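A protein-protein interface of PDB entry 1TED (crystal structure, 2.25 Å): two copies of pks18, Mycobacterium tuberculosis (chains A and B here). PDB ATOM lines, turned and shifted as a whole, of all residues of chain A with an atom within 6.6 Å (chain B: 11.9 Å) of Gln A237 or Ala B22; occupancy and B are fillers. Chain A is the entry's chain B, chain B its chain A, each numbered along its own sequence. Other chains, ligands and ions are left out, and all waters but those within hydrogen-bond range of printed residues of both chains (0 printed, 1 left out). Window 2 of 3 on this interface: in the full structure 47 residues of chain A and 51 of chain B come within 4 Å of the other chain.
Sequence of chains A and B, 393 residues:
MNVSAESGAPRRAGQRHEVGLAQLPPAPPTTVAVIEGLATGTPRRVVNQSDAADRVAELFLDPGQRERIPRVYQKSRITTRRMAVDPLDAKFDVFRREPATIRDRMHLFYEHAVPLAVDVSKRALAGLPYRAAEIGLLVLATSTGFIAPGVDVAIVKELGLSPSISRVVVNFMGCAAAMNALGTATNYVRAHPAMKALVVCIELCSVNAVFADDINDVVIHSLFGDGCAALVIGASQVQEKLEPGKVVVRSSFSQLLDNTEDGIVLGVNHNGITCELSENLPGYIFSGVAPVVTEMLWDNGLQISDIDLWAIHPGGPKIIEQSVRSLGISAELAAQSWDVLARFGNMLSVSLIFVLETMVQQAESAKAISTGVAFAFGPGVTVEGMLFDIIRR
OE1 of Gln A237 sits close to O of Leu B24 (3.1 Å).
N of Val A32 is in hydrogen-bond range of O of Ser A236 (2.6 Å).
The side-chain carboxylate (OE1) of Glu A240 is in hydrogen-bond range of the side-chain hydroxyl (OG) of Ser A236, 2.8 Å away.
Among the printed residues, pairs that only touch across the chains: Ser A236 with Pro B26, Gln A237 with Pro B26, Gln A237 with Ala B22, Thr A31 with Pro B26, Ala A235 with Pro B26 and Glu A240 with Gln B23.
Thr A31 touches just one residue of chain B: Pro B26.
No residue of chain B comes within 4 Å of Val A32.
Ala A235 touches one residue of chain B.
Gln A237 touches three residues of chain B.
No residue of chain B comes within 4 Å of Val A238.
Gln A239 touches none of the printed residues of chain B.
Ala B22 touches just one residue of chain A: Gln A237.
Printed residues of chain A within 4 Å of Gln B23: Glu A240 (3.9 Å).
Of the printed residues of chain A, Leu B24 touches Gln A237.
Of the printed residues of chain A, Pro B26 touches Thr A31, Ala A235, Ser A236 and Gln A237.
The nearest printed residue of chain A that does not touch Leu B24 is Glu A240 (5.0 Å).
Along chain B the printed residues that touch a printed residue of chain A span positions 22 to 26.
Among the printed residues, no Asp or Glu carboxylate lies within 4 Å of a Lys or Arg side-chain nitrogen of the other chain.
No position is printed for both chains.
Of the 7 pairs that touch across the chains among the printed residues, none has its exchanged pair printed and touching as well.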
ATOM      1  N   THR A  31     -12.397 -16.667  25.031  1.00  0.00           N
ATOM      2  CA  THR A  31     -13.498 -15.665  25.103  1.00  0.00           C
ATOM      3  C   THR A  31     -14.896 -16.282  25.053  1.00  0.00           C
ATOM      4  O   THR A  31     -15.166 -17.230  24.311  1.00  0.00           O
ATOM      5  CB  THR A  31     -13.360 -14.598  23.983  1.00  0.00           C
ATOM      6  OG1 THR A  31     -14.637 -14.001  23.724  1.00  0.00           O
ATOM      7  CG2 THR A  31     -12.822 -15.214  22.713  1.00  0.00           C
ATOM      8  N   VAL A  32     -15.785 -15.717  25.856  1.00  0.00           N
ATOM      9  CA  VAL A  32     -17.156 -16.184  25.962  1.00  0.00           C
ATOM     10  C   VAL A  32     -18.178 -15.131  25.529  1.00  0.00           C
ATOM     11  O   VAL A  32     -17.987 -13.944  25.762  1.00  0.00           O
ATOM     12  CB  VAL A  32     -17.426 -16.616  27.421  1.00  0.00           C
ATOM     13  CG1 VAL A  32     -18.900 -16.581  27.723  1.00  0.00           C
ATOM     14  CG2 VAL A  32     -16.871 -18.028  27.646  1.00  0.00           C
ATOM     15  N   ALA A 235     -18.883  -9.770  24.820  1.00  0.00           N
ATOM     16  CA  ALA A 235     -17.838 -10.782  24.895  1.00  0.00           C
ATOM     17  C   ALA A 235     -17.138 -10.640  26.231  1.00  0.00           C
ATOM     18  O   ALA A 235     -17.013  -9.543  26.769  1.00  0.00           O
ATOM     19  CB  ALA A 235     -16.844 -10.607  23.759  1.00  0.00           C
ATOM     20  N   SER A 236     -16.667 -11.752  26.768  1.00  0.00           N
ATOM     21  CA  SER A 236     -16.006 -11.718  28.056  1.00  0.00           C
ATOM     22  C   SER A 236     -14.946 -12.807  28.163  1.00  0.00           C
ATOM     23  O   SER A 236     -15.029 -13.829  27.490  1.00  0.00           O
ATOM     24  CB  SER A 236     -17.068 -11.875  29.156  1.00  0.00           C
ATOM     25  OG  SER A 236     -16.487 -12.143  30.418  1.00  0.00           O
ATOM     26  N   GLN A 237     -13.929 -12.570  28.986  1.00  0.00           N
ATOM     27  CA  GLN A 237     -12.877 -13.559  29.197  1.00  0.00           C
ATOM     28  C   GLN A 237     -13.506 -14.758  29.912  1.00  0.00           C
ATOM     29  O   GLN A 237     -14.559 -14.631  30.535  1.00  0.00           O
ATOM     30  CB  GLN A 237     -11.770 -12.985  30.079  1.00  0.00           C
ATOM     31  CG  GLN A 237     -10.880 -11.950  29.418  1.00  0.00           C
ATOM     32  CD  GLN A 237      -9.846 -11.393  30.386  1.00  0.00           C
ATOM     33  OE1 GLN A 237      -9.923 -10.233  30.794  1.00  0.00           O
ATOM     34  NE2 GLN A 237      -8.883 -12.227  30.770  1.00  0.00           N
ATOM     35  N   VAL A 238     -12.863 -15.919  29.827  1.00  0.00           N
ATOM     36  CA  VAL A 238     -13.386 -17.109  30.485  1.00  0.00           C
ATOM     37  C   VAL A 238     -13.247 -16.939  31.991  1.00  0.00           C
ATOM     38  O   VAL A 238     -14.112 -17.354  32.762  1.00  0.00           O
ATOM     39  CB  VAL A 238     -12.616 -18.382  30.069  1.00  0.00           C
ATOM     40  CG1 VAL A 238     -13.362 -19.620  30.562  1.00  0.00           C
ATOM     41  CG2 VAL A 238     -12.440 -18.417  28.557  1.00  0.00           C
ATOM     42  N   GLN A 239     -12.149 -16.310  32.394  1.00  0.00           N
ATOM     43  CA  GLN A 239     -11.844 -16.068  33.798  1.00  0.00           C
ATOM     44  C   GLN A 239     -12.813 -15.131  34.503  1.00  0.00           C
ATOM     45  O   GLN A 239     -13.013 -15.250  35.711  1.00  0.00           O
ATOM     46  CB  GLN A 239     -10.444 -15.476  33.931  1.00  0.00           C
ATOM     47  CG  GLN A 239      -9.353 -16.301  33.304  1.00  0.00           C
ATOM     48  CD  GLN A 239      -8.035 -15.556  33.243  1.00  0.00           C
ATOM     49  OE1 GLN A 239      -7.561 -15.022  34.251  1.00  0.00           O
ATOM     50  NE2 GLN A 239      -7.431 -15.517  32.056  1.00  0.00           N
ATOM     51  N   GLU A 240     -13.406 -14.191  33.773  1.00  0.00           N
ATOM     52  CA  GLU A 240     -14.307 -13.234  34.411  1.00  0.00           C
ATOM     53  C   GLU A 240     -15.457 -13.903  35.151  1.00  0.00           C
ATOM     54  O   GLU A 240     -16.155 -14.752  34.598  1.00  0.00           O
ATOM     55  CB  GLU A 240     -14.878 -12.246  33.390  1.00  0.00           C
ATOM     56  CG  GLU A 240     -15.384 -10.954  34.024  1.00  0.00           C
ATOM     57  CD  GLU A 240     -16.221 -10.113  33.080  1.00  0.00           C
ATOM     58  OE1 GLU A 240     -15.802  -9.898  31.923  1.00  0.00           O
ATOM     59  OE2 GLU A 240     -17.301  -9.655  33.499  1.00  0.00           O
ATOM     60  N   LYS A 241     -15.641 -13.525  36.413  1.00  0.00           N
ATOM     61  CA  LYS A 241     -16.727 -14.081  37.200  1.00  0.00           C
ATOM     62  C   LYS A 241     -17.961 -13.237  36.932  1.00  0.00           C
ATOM     63  O   LYS A 241     -18.073 -12.100  37.387  1.00  0.00           O
ATOM     64  CB  LYS A 241     -16.370 -14.087  38.687  1.00  0.00           C
ATOM     65  CG  LYS A 241     -15.247 -15.063  38.997  1.00  0.00           C
ATOM     66  CD  LYS A 241     -14.950 -15.167  40.486  1.00  0.00           C
ATOM     67  CE  LYS A 241     -13.813 -16.159  40.745  1.00  0.00           C
ATOM     68  NZ  LYS A 241     -13.478 -16.283  42.200  1.00  0.00           N
ATOM     69  N   LEU A 242     -18.873 -13.812  36.160  1.00  0.00           N
ATOM     70  CA  LEU A 242     -20.109 -13.151  35.777  1.00  0.00           C
ATOM     71  C   LEU A 242     -21.096 -13.043  36.934  1.00  0.00           C
ATOM     72  O   LEU A 242     -21.092 -13.876  37.843  1.00  0.00           O
ATOM     73  CB  LEU A 242     -20.746 -13.924  34.622  1.00  0.00           C
ATOM     74  CG  LEU A 242     -19.861 -14.119  33.393  1.00  0.00           C
ATOM     75  CD1 LEU A 242     -20.519 -15.078  32.431  1.00  0.00           C
ATOM     76  CD2 LEU A 242     -19.611 -12.761  32.742  1.00  0.00           C
ATOM     77  N   ALA B  22      -8.911  -7.755  36.869  1.00  0.00           N
ATOM     78  CA  ALA B  22      -8.817  -7.385  35.430  1.00  0.00           C
ATOM     79  C   ALA B  22      -9.941  -8.040  34.621  1.00  0.00           C
ATOM     80  O   ALA B  22      -9.857  -9.219  34.250  1.00  0.00           O
ATOM     81  CB  ALA B  22      -7.454  -7.794  34.873  1.00  0.00           C
ATOM     82  N   GLN B  23     -10.989  -7.258  34.359  1.00  0.00           N
ATOM     83  CA  GLN B  23     -12.156  -7.702  33.594  1.00  0.00           C
ATOM     84  C   GLN B  23     -12.158  -7.081  32.192  1.00  0.00           C
ATOM     85  O   GLN B  23     -13.202  -6.975  31.550  1.00  0.00           O
ATOM     86  CB  GLN B  23     -13.432  -7.303  34.337  1.00  0.00           C
ATOM     87  CG  GLN B  23     -13.474  -7.829  35.761  1.00  0.00           C
ATOM     88  CD  GLN B  23     -14.465  -7.088  36.628  1.00  0.00           C
ATOM     89  OE1 GLN B  23     -14.370  -5.868  36.791  1.00  0.00           O
ATOM     90  NE2 GLN B  23     -15.421  -7.819  37.196  1.00  0.00           N
ATOM     91  N   LEU B  24     -10.979  -6.666  31.736  1.00  0.00           N
ATOM     92  CA  LEU B  24     -10.795  -6.064  30.418  1.00  0.00           C
ATOM     93  C   LEU B  24     -11.461  -6.911  29.340  1.00  0.00           C
ATOM     94  O   LEU B  24     -11.749  -8.087  29.554  1.00  0.00           O
ATOM     95  CB  LEU B  24      -9.306  -5.971  30.098  1.00  0.00           C
ATOM     96  CG  LEU B  24      -8.403  -5.083  30.953  1.00  0.00           C
ATOM     97  CD1 LEU B  24      -6.956  -5.544  30.820  1.00  0.00           C
ATOM     98  CD2 LEU B  24      -8.557  -3.631  30.510  1.00  0.00           C
ATOM     99  N   PRO B  25     -11.705  -6.326  28.159  1.00  0.00           N
ATOM    100  CA  PRO B  25     -12.336  -7.095  27.084  1.00  0.00           C
ATOM    101  C   PRO B  25     -11.331  -8.102  26.549  1.00  0.00           C
ATOM    102  O   PRO B  25     -10.121  -7.864  26.587  1.00  0.00           O
ATOM    103  CB  PRO B  25     -12.660  -6.036  26.035  1.00  0.00           C
ATOM    104  CG  PRO B  25     -12.702  -4.755  26.806  1.00  0.00           C
ATOM    105  CD  PRO B  25     -11.568  -4.912  27.777  1.00  0.00           C
ATOM    106  N   PRO B  26     -11.813  -9.250  26.055  1.00  0.00           N
ATOM    107  CA  PRO B  26     -10.908 -10.268  25.512  1.00  0.00           C
ATOM    108  C   PRO B  26     -10.150  -9.680  24.320  1.00  0.00           C
ATOM    109  O   PRO B  26     -10.651  -8.785  23.655  1.00  0.00           O
ATOM    110  CB  PRO B  26     -11.861 -11.375  25.062  1.00  0.00           C
ATOM    111  CG  PRO B  26     -13.063 -11.186  25.940  1.00  0.00           C
ATOM    112  CD  PRO B  26     -13.215  -9.699  26.002  1.00  0.00           C
ATOM    113  N   ALA B  27      -8.954 -10.187  24.050  1.00  0.00           N
ATOM    114  CA  ALA B  27      -8.163  -9.716  22.917  1.00  0.00           C
ATOM    115  C   ALA B  27      -8.904 -10.050  21.622  1.00  0.00           C
ATOM    116  O   ALA B  27      -9.496 -11.116  21.496  1.00  0.00           O
ATOM    117  CB  ALA B  27      -6.782 -10.392  22.916  1.00  0.00           C
ATOM    118  N   PRO B  28      -8.871  -9.141  20.637  1.00  0.00           N
ATOM    119  CA  PRO B  28      -9.539  -9.333  19.346  1.00  0.00           C
ATOM    120  C   PRO B  28      -8.804 -10.317  18.436  1.00  0.00           C
ATOM    121  O   PRO B  28      -7.595 -10.494  18.555  1.00  0.00           O
ATOM    122  CB  PRO B  28      -9.506  -7.939  18.706  1.00  0.00           C
ATOM    123  CG  PRO B  28      -9.007  -7.022  19.786  1.00  0.00           C
ATOM    124  CD  PRO B  28      -8.138  -7.870  20.648  1.00  0.00           C
